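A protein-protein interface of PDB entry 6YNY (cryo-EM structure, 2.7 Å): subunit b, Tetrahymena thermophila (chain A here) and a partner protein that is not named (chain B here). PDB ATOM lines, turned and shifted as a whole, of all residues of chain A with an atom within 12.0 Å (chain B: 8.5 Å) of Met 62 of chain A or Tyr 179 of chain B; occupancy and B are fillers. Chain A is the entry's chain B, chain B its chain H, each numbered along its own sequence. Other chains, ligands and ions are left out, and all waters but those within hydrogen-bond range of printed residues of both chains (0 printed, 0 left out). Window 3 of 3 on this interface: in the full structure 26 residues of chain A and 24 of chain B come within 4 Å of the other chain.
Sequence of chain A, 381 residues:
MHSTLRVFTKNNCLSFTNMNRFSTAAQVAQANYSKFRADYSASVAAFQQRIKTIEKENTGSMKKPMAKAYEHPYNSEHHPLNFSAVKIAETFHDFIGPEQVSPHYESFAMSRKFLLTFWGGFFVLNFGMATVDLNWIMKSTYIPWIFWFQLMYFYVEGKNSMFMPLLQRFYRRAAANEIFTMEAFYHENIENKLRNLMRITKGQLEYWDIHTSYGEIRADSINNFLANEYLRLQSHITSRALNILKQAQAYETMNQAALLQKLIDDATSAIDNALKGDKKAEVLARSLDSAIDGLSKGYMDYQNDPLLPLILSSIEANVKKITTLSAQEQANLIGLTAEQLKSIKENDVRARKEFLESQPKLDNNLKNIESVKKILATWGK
The backbone carbonyl oxygen (O) of Met 66 of chain A sits at hydrogen-bond distance from the side-chain amide nitrogen (ND2) of Asn 176 of chain B (3.2 Å).
ND2 of Asn 176 of chain B lies within hydrogen-bond range of O of Leu 172 of chain B (3.2 Å).
Among the printed residues, merely in contact across the chains: Met 62 of chain A with Lys 175 of chain B (3.5 Å), Met 62 of chain A with Tyr 179 of chain B (3.8 Å), Met 62 of chain A with Ile 182 of chain B (3.6 Å), Lys 63 of chain A with Tyr 179 of chain B (3.6 Å), Lys 64 of chain A with Tyr 179 of chain B (3.5 Å), Pro 65 of chain A with Asn 176 of chain B (3.2 Å), Met 66 of chain A with Leu 172 of chain B (3.96 Å), Ala 67 of chain A with Asn 176 of chain B (3.6 Å) and Lys 68 of chain A with Leu 172 of chain B (3.8 Å).
Of chain B, only Lys 175 (3.5 Å), Tyr 179 (3.8 Å) and Ile 182 (3.6 Å) come within 4 Å of Met 62 of chain A. Of chain A, only Met 62, Lys 63 and Lys 64 come within 4 Å of Tyr 179 of chain B. Asn 176 of chain B touches three residues of chain A. No residue of chain A comes within 4 Å of Glu 180 of chain B. Ile 182 of chain B touches one residue of chain A. No residue of chain A comes within 4 Å of Gln 183 of chain B. Printed residues of chain B within 4 Å of Ala 67 of chain A: Asn 176 (3.6 Å). Of the printed residues of chain B, Pro 65 of chain A touches Asn 176. The nearest residue of chain B that does not touch Met 62 of chain A is Gln 178 of chain B (4.3 Å). The nearest residue of chain A that does not touch Tyr 179 of chain B is Pro 65 of chain A (4.2 Å). The nearest printed residue of chain B that does not touch Ala 67 of chain A is Leu 172 of chain B (4.6 Å).
Of the 13 printed residues of chain A, 7 touch a printed residue of chain B. Hydrophobic or aromatic side chains of chain A within 4 Å of the printed part of chain B: Met 62 and Pro 65. Hydrophobic or aromatic side chains of chain B that line the printed part of chain A: Leu 172, Tyr 179 and Ile 182. Among the printed residues, 10 pairs touch across the chains. Among the printed residues, no Asp or Glu carboxylate lies within 4 Å of a Lys or Arg side-chain nitrogen of the other chain.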
ATOM      1  N   LYS A  56       6.462   9.810 -13.761  1.00  0.00           N
ATOM      2  CA  LYS A  56       5.449   8.766 -13.860  1.00  0.00           C
ATOM      3  C   LYS A  56       5.194   8.392 -15.312  1.00  0.00           C
ATOM      4  O   LYS A  56       4.992   7.216 -15.635  1.00  0.00           O
ATOM      5  CB  LYS A  56       4.158   9.229 -13.187  1.00  0.00           C
ATOM      6  CG  LYS A  56       4.334   9.596 -11.725  1.00  0.00           C
ATOM      7  CD  LYS A  56       3.057  10.147 -11.114  1.00  0.00           C
ATOM      8  CE  LYS A  56       1.988   9.072 -10.982  1.00  0.00           C
ATOM      9  NZ  LYS A  56       0.764   9.570 -10.294  1.00  0.00           N
ATOM     10  N   GLU A  57       5.201   9.384 -16.205  1.00  0.00           N
ATOM     11  CA  GLU A  57       4.981   9.112 -17.619  1.00  0.00           C
ATOM     12  C   GLU A  57       6.132   8.320 -18.220  1.00  0.00           C
ATOM     13  O   GLU A  57       5.915   7.489 -19.110  1.00  0.00           O
ATOM     14  CB  GLU A  57       4.784  10.424 -18.375  1.00  0.00           C
ATOM     15  CG  GLU A  57       3.512  11.162 -18.002  1.00  0.00           C
ATOM     16  CD  GLU A  57       2.260  10.418 -18.426  1.00  0.00           C
ATOM     17  OE1 GLU A  57       2.377   9.451 -19.208  1.00  0.00           O
ATOM     18  OE2 GLU A  57       1.160  10.799 -17.975  1.00  0.00           O
ATOM     19  N   ASN A  58       7.357   8.561 -17.751  1.00  0.00           N
ATOM     20  CA  ASN A  58       8.513   7.850 -18.281  1.00  0.00           C
ATOM     21  C   ASN A  58       8.430   6.353 -18.017  1.00  0.00           C
ATOM     22  O   ASN A  58       9.054   5.571 -18.744  1.00  0.00           O
ATOM     23  CB  ASN A  58       9.795   8.418 -17.674  1.00  0.00           C
ATOM     24  CG  ASN A  58      11.042   7.890 -18.350  1.00  0.00           C
ATOM     25  OD1 ASN A  58      11.575   6.847 -17.969  1.00  0.00           O
ATOM     26  ND2 ASN A  58      11.516   8.610 -19.361  1.00  0.00           N
ATOM     27  N   THR A  59       7.674   5.939 -17.000  1.00  0.00           N
ATOM     28  CA  THR A  59       7.524   4.528 -16.667  1.00  0.00           C
ATOM     29  C   THR A  59       6.642   3.774 -17.653  1.00  0.00           C
ATOM     30  O   THR A  59       6.495   2.554 -17.512  1.00  0.00           O
ATOM     31  CB  THR A  59       6.940   4.382 -15.259  1.00  0.00           C
ATOM     32  OG1 THR A  59       5.578   4.825 -15.258  1.00  0.00           O
ATOM     33  CG2 THR A  59       7.734   5.211 -14.259  1.00  0.00           C
ATOM     34  N   GLY A  60       6.051   4.456 -18.630  1.00  0.00           N
ATOM     35  CA  GLY A  60       5.157   3.819 -19.576  1.00  0.00           C
ATOM     36  C   GLY A  60       5.752   2.619 -20.286  1.00  0.00           C
ATOM     37  O   GLY A  60       6.939   2.611 -20.624  1.00  0.00           O
ATOM     38  N   SER A  61       4.928   1.599 -20.515  1.00  0.00           N
ATOM     39  CA  SER A  61       5.317   0.390 -21.230  1.00  0.00           C
ATOM     40  C   SER A  61       4.300   0.128 -22.337  1.00  0.00           C
ATOM     41  O   SER A  61       3.335   0.877 -22.512  1.00  0.00           O
ATOM     42  CB  SER A  61       5.421  -0.810 -20.280  1.00  0.00           C
ATOM     43  OG  SER A  61       4.191  -1.047 -19.617  1.00  0.00           O
ATOM     44  N   MET A  62       4.519  -0.950 -23.088  1.00  0.00           N
ATOM     45  CA  MET A  62       3.693  -1.279 -24.240  1.00  0.00           C
ATOM     46  C   MET A  62       3.194  -2.712 -24.139  1.00  0.00           C
ATOM     47  O   MET A  62       3.882  -3.593 -23.618  1.00  0.00           O
ATOM     48  CB  MET A  62       4.472  -1.103 -25.544  1.00  0.00           C
ATOM     49  CG  MET A  62       3.631  -1.253 -26.792  1.00  0.00           C
ATOM     50  SD  MET A  62       4.602  -1.120 -28.301  1.00  0.00           S
ATOM     51  CE  MET A  62       3.305  -1.137 -29.529  1.00  0.00           C
ATOM     52  N   LYS A  63       1.989  -2.934 -24.654  1.00  0.00           N
ATOM     53  CA  LYS A  63       1.396  -4.261 -24.712  1.00  0.00           C
ATOM     54  C   LYS A  63       1.706  -4.917 -26.049  1.00  0.00           C
ATOM     55  O   LYS A  63       1.859  -4.245 -27.072  1.00  0.00           O
ATOM     56  CB  LYS A  63      -0.117  -4.186 -24.525  1.00  0.00           C
ATOM     57  CG  LYS A  63      -0.554  -3.678 -23.168  1.00  0.00           C
ATOM     58  CD  LYS A  63      -2.066  -3.533 -23.092  1.00  0.00           C
ATOM     59  CE  LYS A  63      -2.770  -4.876 -23.214  1.00  0.00           C
ATOM     60  NZ  LYS A  63      -4.238  -4.744 -23.022  1.00  0.00           N
ATOM     61  N   LYS A  64       1.788  -6.237 -26.035  1.00  0.00           N
ATOM     62  CA  LYS A  64       2.063  -6.970 -27.262  1.00  0.00           C
ATOM     63  C   LYS A  64       0.816  -6.997 -28.133  1.00  0.00           C
ATOM     64  O   LYS A  64      -0.222  -7.510 -27.695  1.00  0.00           O
ATOM     65  CB  LYS A  64       2.521  -8.386 -26.952  1.00  0.00           C
ATOM     66  CG  LYS A  64       2.877  -9.174 -28.188  1.00  0.00           C
ATOM     67  CD  LYS A  64       3.638 -10.430 -27.848  1.00  0.00           C
ATOM     68  CE  LYS A  64       4.079 -11.156 -29.101  1.00  0.00           C
ATOM     69  NZ  LYS A  64       4.929 -12.334 -28.792  1.00  0.00           N
ATOM     70  N   PRO A  65       0.860  -6.473 -29.351  1.00  0.00           N
ATOM     71  CA  PRO A  65      -0.324  -6.468 -30.210  1.00  0.00           C
ATOM     72  C   PRO A  65      -0.501  -7.817 -30.898  1.00  0.00           C
ATOM     73  O   PRO A  65       0.312  -8.727 -30.763  1.00  0.00           O
ATOM     74  CB  PRO A  65      -0.011  -5.359 -31.210  1.00  0.00           C
ATOM     75  CG  PRO A  65       1.457  -5.416 -31.351  1.00  0.00           C
ATOM     76  CD  PRO A  65       2.002  -5.816 -30.007  1.00  0.00           C
ATOM     77  N   MET A  66      -1.592  -7.927 -31.649  1.00  0.00           N
ATOM     78  CA  MET A  66      -1.859  -9.152 -32.384  1.00  0.00           C
ATOM     79  C   MET A  66      -0.796  -9.374 -33.451  1.00  0.00           C
ATOM     80  O   MET A  66      -0.217  -8.431 -33.994  1.00  0.00           O
ATOM     81  CB  MET A  66      -3.242  -9.095 -33.025  1.00  0.00           C
ATOM     82  CG  MET A  66      -4.377  -9.048 -32.029  1.00  0.00           C
ATOM     83  SD  MET A  66      -5.984  -8.934 -32.821  1.00  0.00           S
ATOM     84  CE  MET A  66      -5.969 -10.426 -33.804  1.00  0.00           C
ATOM     85  N   ALA A  67      -0.546 -10.647 -33.752  1.00  0.00           N
ATOM     86  CA  ALA A  67       0.497 -10.988 -34.710  1.00  0.00           C
ATOM     87  C   ALA A  67       0.103 -10.594 -36.126  1.00  0.00           C
ATOM     88  O   ALA A  67       0.927 -10.066 -36.882  1.00  0.00           O
ATOM     89  CB  ALA A  67       0.800 -12.481 -34.636  1.00  0.00           C
ATOM     90  N   LYS A  68      -1.147 -10.841 -36.506  1.00  0.00           N
ATOM     91  CA  LYS A  68      -1.592 -10.575 -37.864  1.00  0.00           C
ATOM     92  C   LYS A  68      -3.108 -10.639 -37.912  1.00  0.00           C
ATOM     93  O   LYS A  68      -3.753 -11.202 -37.024  1.00  0.00           O
ATOM     94  CB  LYS A  68      -0.997 -11.577 -38.854  1.00  0.00           C
ATOM     95  CG  LYS A  68      -1.266 -13.025 -38.482  1.00  0.00           C
ATOM     96  CD  LYS A  68      -1.010 -13.968 -39.640  1.00  0.00           C
ATOM     97  CE  LYS A  68      -2.137 -13.906 -40.661  1.00  0.00           C
ATOM     98  NZ  LYS A  68      -2.002 -14.947 -41.708  1.00  0.00           N
ATOM     99  N   HIS B 171      -1.180  -2.178 -40.341  1.00  0.00           N
ATOM    100  CA  HIS B 171      -1.118  -1.483 -39.062  1.00  0.00           C
ATOM    101  C   HIS B 171      -0.421  -2.324 -38.002  1.00  0.00           C
ATOM    102  O   HIS B 171       0.411  -1.811 -37.249  1.00  0.00           O
ATOM    103  CB  HIS B 171      -2.528  -1.120 -38.607  1.00  0.00           C
ATOM    104  CG  HIS B 171      -2.572  -0.306 -37.353  1.00  0.00           C
ATOM    105  ND1 HIS B 171      -2.132   0.998 -37.298  1.00  0.00           N
ATOM    106  CD2 HIS B 171      -3.012  -0.609 -36.110  1.00  0.00           C
ATOM    107  CE1 HIS B 171      -2.295   1.462 -36.073  1.00  0.00           C
ATOM    108  NE2 HIS B 171      -2.828   0.507 -35.332  1.00  0.00           N
ATOM    109  N   LEU B 172      -0.748  -3.615 -37.933  1.00  0.00           N
ATOM    110  CA  LEU B 172      -0.154  -4.476 -36.920  1.00  0.00           C
ATOM    111  C   LEU B 172       1.328  -4.695 -37.169  1.00  0.00           C
ATOM    112  O   LEU B 172       2.102  -4.837 -36.216  1.00  0.00           O
ATOM    113  CB  LEU B 172      -0.887  -5.812 -36.883  1.00  0.00           C
ATOM    114  CG  LEU B 172      -2.367  -5.721 -36.533  1.00  0.00           C
ATOM    115  CD1 LEU B 172      -3.030  -7.062 -36.686  1.00  0.00           C
ATOM    116  CD2 LEU B 172      -2.537  -5.205 -35.126  1.00  0.00           C
ATOM    117  N   ALA B 173       1.740  -4.731 -38.434  1.00  0.00           N
ATOM    118  CA  ALA B 173       3.156  -4.870 -38.741  1.00  0.00           C
ATOM    119  C   ALA B 173       3.958  -3.703 -38.189  1.00  0.00           C
ATOM    120  O   ALA B 173       5.104  -3.880 -37.766  1.00  0.00           O
ATOM    121  CB  ALA B 173       3.348  -4.977 -40.248  1.00  0.00           C
ATOM    122  N   TRP B 174       3.372  -2.507 -38.186  1.00  0.00           N
ATOM    123  CA  TRP B 174       4.059  -1.332 -37.675  1.00  0.00           C
ATOM    124  C   TRP B 174       4.019  -1.272 -36.156  1.00  0.00           C
ATOM    125  O   TRP B 174       4.952  -0.753 -35.536  1.00  0.00           O
ATOM    126  CB  TRP B 174       3.439  -0.076 -38.284  1.00  0.00           C
ATOM    127  CG  TRP B 174       3.994   1.201 -37.767  1.00  0.00           C
ATOM    128  CD1 TRP B 174       5.300   1.582 -37.753  1.00  0.00           C
ATOM    129  CD2 TRP B 174       3.253   2.289 -37.208  1.00  0.00           C
ATOM    130  NE1 TRP B 174       5.423   2.835 -37.210  1.00  0.00           N
ATOM    131  CE2 TRP B 174       4.178   3.292 -36.868  1.00  0.00           C
ATOM    132  CE3 TRP B 174       1.898   2.511 -36.958  1.00  0.00           C
ATOM    133  CZ2 TRP B 174       3.792   4.494 -36.291  1.00  0.00           C
ATOM    134  CZ3 TRP B 174       1.518   3.705 -36.386  1.00  0.00           C
ATOM    135  CH2 TRP B 174       2.461   4.682 -36.058  1.00  0.00           C
ATOM    136  N   LYS B 175       2.957  -1.797 -35.542  1.00  0.00           N
ATOM    137  CA  LYS B 175       2.906  -1.863 -34.087  1.00  0.00           C
ATOM    138  C   LYS B 175       3.827  -2.947 -33.546  1.00  0.00           C
ATOM    139  O   LYS B 175       4.367  -2.804 -32.445  1.00  0.00           O
ATOM    140  CB  LYS B 175       1.472  -2.103 -33.624  1.00  0.00           C
ATOM    141  CG  LYS B 175       0.607  -0.863 -33.641  1.00  0.00           C
ATOM    142  CD  LYS B 175       0.920   0.049 -32.473  1.00  0.00           C
ATOM    143  CE  LYS B 175       0.151   1.350 -32.557  1.00  0.00           C
ATOM    144  NZ  LYS B 175       0.587   2.172 -33.716  1.00  0.00           N
ATOM    145  N   ASN B 176       4.012  -4.034 -34.294  1.00  0.00           N
ATOM    146  CA  ASN B 176       4.951  -5.066 -33.874  1.00  0.00           C
ATOM    147  C   ASN B 176       6.391  -4.607 -34.041  1.00  0.00           C
ATOM    148  O   ASN B 176       7.259  -4.994 -33.251  1.00  0.00           O
ATOM    149  CB  ASN B 176       4.704  -6.349 -34.660  1.00  0.00           C
ATOM    150  CG  ASN B 176       3.580  -7.174 -34.080  1.00  0.00           C
ATOM    151  OD1 ASN B 176       3.489  -7.352 -32.867  1.00  0.00           O
ATOM    152  ND2 ASN B 176       2.713  -7.680 -34.944  1.00  0.00           N
ATOM    153  N   GLU B 177       6.664  -3.789 -35.057  1.00  0.00           N
ATOM    154  CA  GLU B 177       8.003  -3.237 -35.217  1.00  0.00           C
ATOM    155  C   GLU B 177       8.366  -2.349 -34.037  1.00  0.00           C
ATOM    156  O   GLU B 177       9.524  -2.316 -33.605  1.00  0.00           O
ATOM    157  CB  GLU B 177       8.091  -2.460 -36.528  1.00  0.00           C
ATOM    158  CG  GLU B 177       9.442  -1.826 -36.789  1.00  0.00           C
ATOM    159  CD  GLU B 177       9.507  -1.130 -38.133  1.00  0.00           C
ATOM    160  OE1 GLU B 177       8.500  -1.162 -38.868  1.00  0.00           O
ATOM    161  OE2 GLU B 177      10.567  -0.552 -38.452  1.00  0.00           O
ATOM    162  N   GLN B 178       7.387  -1.615 -33.504  1.00  0.00           N
ATOM    163  CA  GLN B 178       7.632  -0.801 -32.321  1.00  0.00           C
ATOM    164  C   GLN B 178       7.837  -1.669 -31.088  1.00  0.00           C
ATOM    165  O   GLN B 178       8.713  -1.389 -30.262  1.00  0.00           O
ATOM    166  CB  GLN B 178       6.471   0.164 -32.103  1.00  0.00           C
ATOM    167  CG  GLN B 178       6.327   1.214 -33.178  1.00  0.00           C
ATOM    168  CD  GLN B 178       5.194   2.173 -32.894  1.00  0.00           C
ATOM    169  OE1 GLN B 178       4.085   1.761 -32.558  1.00  0.00           O
ATOM    170  NE2 GLN B 178       5.470   3.464 -33.017  1.00  0.00           N
ATOM    171  N   TYR B 179       7.037  -2.725 -30.947  1.00  0.00           N
ATOM    172  CA  TYR B 179       7.154  -3.595 -29.784  1.00  0.00           C
ATOM    173  C   TYR B 179       8.521  -4.261 -29.733  1.00  0.00           C
ATOM    174  O   TYR B 179       9.142  -4.341 -28.668  1.00  0.00           O
ATOM    175  CB  TYR B 179       6.045  -4.642 -29.816  1.00  0.00           C
ATOM    176  CG  TYR B 179       5.974  -5.520 -28.592  1.00  0.00           C
ATOM    177  CD1 TYR B 179       5.370  -5.072 -27.429  1.00  0.00           C
ATOM    178  CD2 TYR B 179       6.497  -6.803 -28.604  1.00  0.00           C
ATOM    179  CE1 TYR B 179       5.298  -5.871 -26.310  1.00  0.00           C
ATOM    180  CE2 TYR B 179       6.429  -7.610 -27.492  1.00  0.00           C
ATOM    181  CZ  TYR B 179       5.828  -7.140 -26.346  1.00  0.00           C
ATOM    182  OH  TYR B 179       5.760  -7.943 -25.233  1.00  0.00           O
ATOM    183  N   GLU B 180       9.011  -4.742 -30.875  1.00  0.00           N
ATOM    184  CA  GLU B 180      10.315  -5.392 -30.901  1.00  0.00           C
ATOM    185  C   GLU B 180      11.435  -4.419 -30.562  1.00  0.00           C
ATOM    186  O   GLU B 180      12.450  -4.821 -29.983  1.00  0.00           O
ATOM    187  CB  GLU B 180      10.555  -6.021 -32.271  1.00  0.00           C
ATOM    188  CG  GLU B 180       9.611  -7.163 -32.586  1.00  0.00           C
ATOM    189  CD  GLU B 180       9.763  -7.674 -34.004  1.00  0.00           C
ATOM    190  OE1 GLU B 180      10.605  -7.127 -34.747  1.00  0.00           O
ATOM    191  OE2 GLU B 180       9.039  -8.621 -34.377  1.00  0.00           O
ATOM    192  N   LYS B 181      11.272  -3.142 -30.910  1.00  0.00           N
ATOM    193  CA  LYS B 181      12.285  -2.147 -30.585  1.00  0.00           C
ATOM    194  C   LYS B 181      12.226  -1.737 -29.121  1.00  0.00           C
ATOM    195  O   LYS B 181      13.252  -1.360 -28.544  1.00  0.00           O
ATOM    196  CB  LYS B 181      12.110  -0.920 -31.477  1.00  0.00           C
ATOM    197  CG  LYS B 181      12.364  -1.193 -32.945  1.00  0.00           C
ATOM    198  CD  LYS B 181      11.833  -0.081 -33.834  1.00  0.00           C
ATOM    199  CE  LYS B 181      12.507   1.247 -33.558  1.00  0.00           C
ATOM    200  NZ  LYS B 181      13.970   1.189 -33.780  1.00  0.00           N
ATOM    201  N   ILE B 182      11.046  -1.801 -28.508  1.00  0.00           N
ATOM    202  CA  ILE B 182      10.913  -1.438 -27.103  1.00  0.00           C
ATOM    203  C   ILE B 182      11.417  -2.559 -26.206  1.00  0.00           C
ATOM    204  O   ILE B 182      12.057  -2.306 -25.179  1.00  0.00           O
ATOM    205  CB  ILE B 182       9.451  -1.075 -26.795  1.00  0.00           C
ATOM    206  CG1 ILE B 182       9.108   0.268 -27.439  1.00  0.00           C
ATOM    207  CG2 ILE B 182       9.217  -1.040 -25.297  1.00  0.00           C
ATOM    208  CD1 ILE B 182       7.639   0.595 -27.434  1.00  0.00           C
ATOM    209  N   GLN B 183      11.138  -3.812 -26.570  1.00  0.00           N
ATOM    210  CA  GLN B 183      11.641  -4.932 -25.783  1.00  0.00           C
ATOM    211  C   GLN B 183      13.161  -4.967 -25.781  1.00  0.00           C
ATOM    212  O   GLN B 183      13.772  -5.421 -24.807  1.00  0.00           O
ATOM    213  CB  GLN B 183      11.080  -6.246 -26.323  1.00  0.00           C
ATOM    214  CG  GLN B 183       9.570  -6.348 -26.243  1.00  0.00           C
ATOM    215  CD  GLN B 183       9.060  -6.369 -24.820  1.00  0.00           C
ATOM    216  OE1 GLN B 183       8.271  -5.513 -24.419  1.00  0.00           O
ATOM    217  NE2 GLN B 183       9.503  -7.351 -24.048  1.00  0.00           N
ATOM    218  N   LYS B 184      13.785  -4.494 -26.855  1.00  0.00           N
ATOM    219  CA  LYS B 184      15.235  -4.395 -26.942  1.00  0.00           C
ATOM    220  C   LYS B 184      15.783  -3.157 -26.248  1.00  0.00           C
ATOM    221  O   LYS B 184      16.984  -2.888 -26.351  1.00  0.00           O
ATOM    222  CB  LYS B 184      15.670  -4.386 -28.407  1.00  0.00           C
ATOM    223  CG  LYS B 184      15.383  -5.673 -29.150  1.00  0.00           C
ATOM    224  CD  LYS B 184      15.511  -5.484 -30.653  1.00  0.00           C
ATOM    225  CE  LYS B 184      16.906  -5.033 -31.047  1.00  0.00           C
ATOM    226  NZ  LYS B 184      17.057  -4.915 -32.524  1.00  0.00           N
ATOM    227  N   GLY B 185      14.939  -2.398 -25.552  1.00  0.00           N
ATOM    228  CA  GLY B 185      15.363  -1.161 -24.938  1.00  0.00           C
ATOM    229  C   GLY B 185      15.639  -0.034 -25.905  1.00  0.00           C
ATOM    230  O   GLY B 185      15.983   1.068 -25.462  1.00  0.00           O
ATOM    231  N   GLU B 186      15.500  -0.269 -27.205  1.00  0.00           N
ATOM    232  CA  GLU B 186      15.747   0.759 -28.199  1.00  0.00           C
ATOM    233  C   GLU B 186      14.599   1.761 -28.226  1.00  0.00           C
ATOM    234  O   GLU B 186      13.478   1.481 -27.792  1.00  0.00           O
ATOM    235  CB  GLU B 186      15.929   0.126 -29.578  1.00  0.00           C
ATOM    236  CG  GLU B 186      16.330   1.099 -30.670  1.00  0.00           C
ATOM    237  CD  GLU B 186      16.645   0.402 -31.978  1.00  0.00           C
ATOM    238  OE1 GLU B 186      16.588  -0.845 -32.017  1.00  0.00           O
ATOM    239  OE2 GLU B 186      16.949   1.099 -32.967  1.00  0.00           O
ATOM    240  N   THR B 188      11.975   4.260 -30.226  1.00  0.00           N
ATOM    241  CA  THR B 188      11.235   4.280 -31.477  1.00  0.00           C
ATOM    242  C   THR B 188      11.406   5.616 -32.185  1.00  0.00           C
ATOM    243  O   THR B 188      11.674   6.648 -31.564  1.00  0.00           O
ATOM    244  CB  THR B 188       9.749   4.026 -31.231  1.00  0.00           C
ATOM    245  OG1 THR B 188       9.189   5.114 -30.489  1.00  0.00           O
ATOM    246  CG2 THR B 188       9.548   2.746 -30.460  1.00  0.00           C
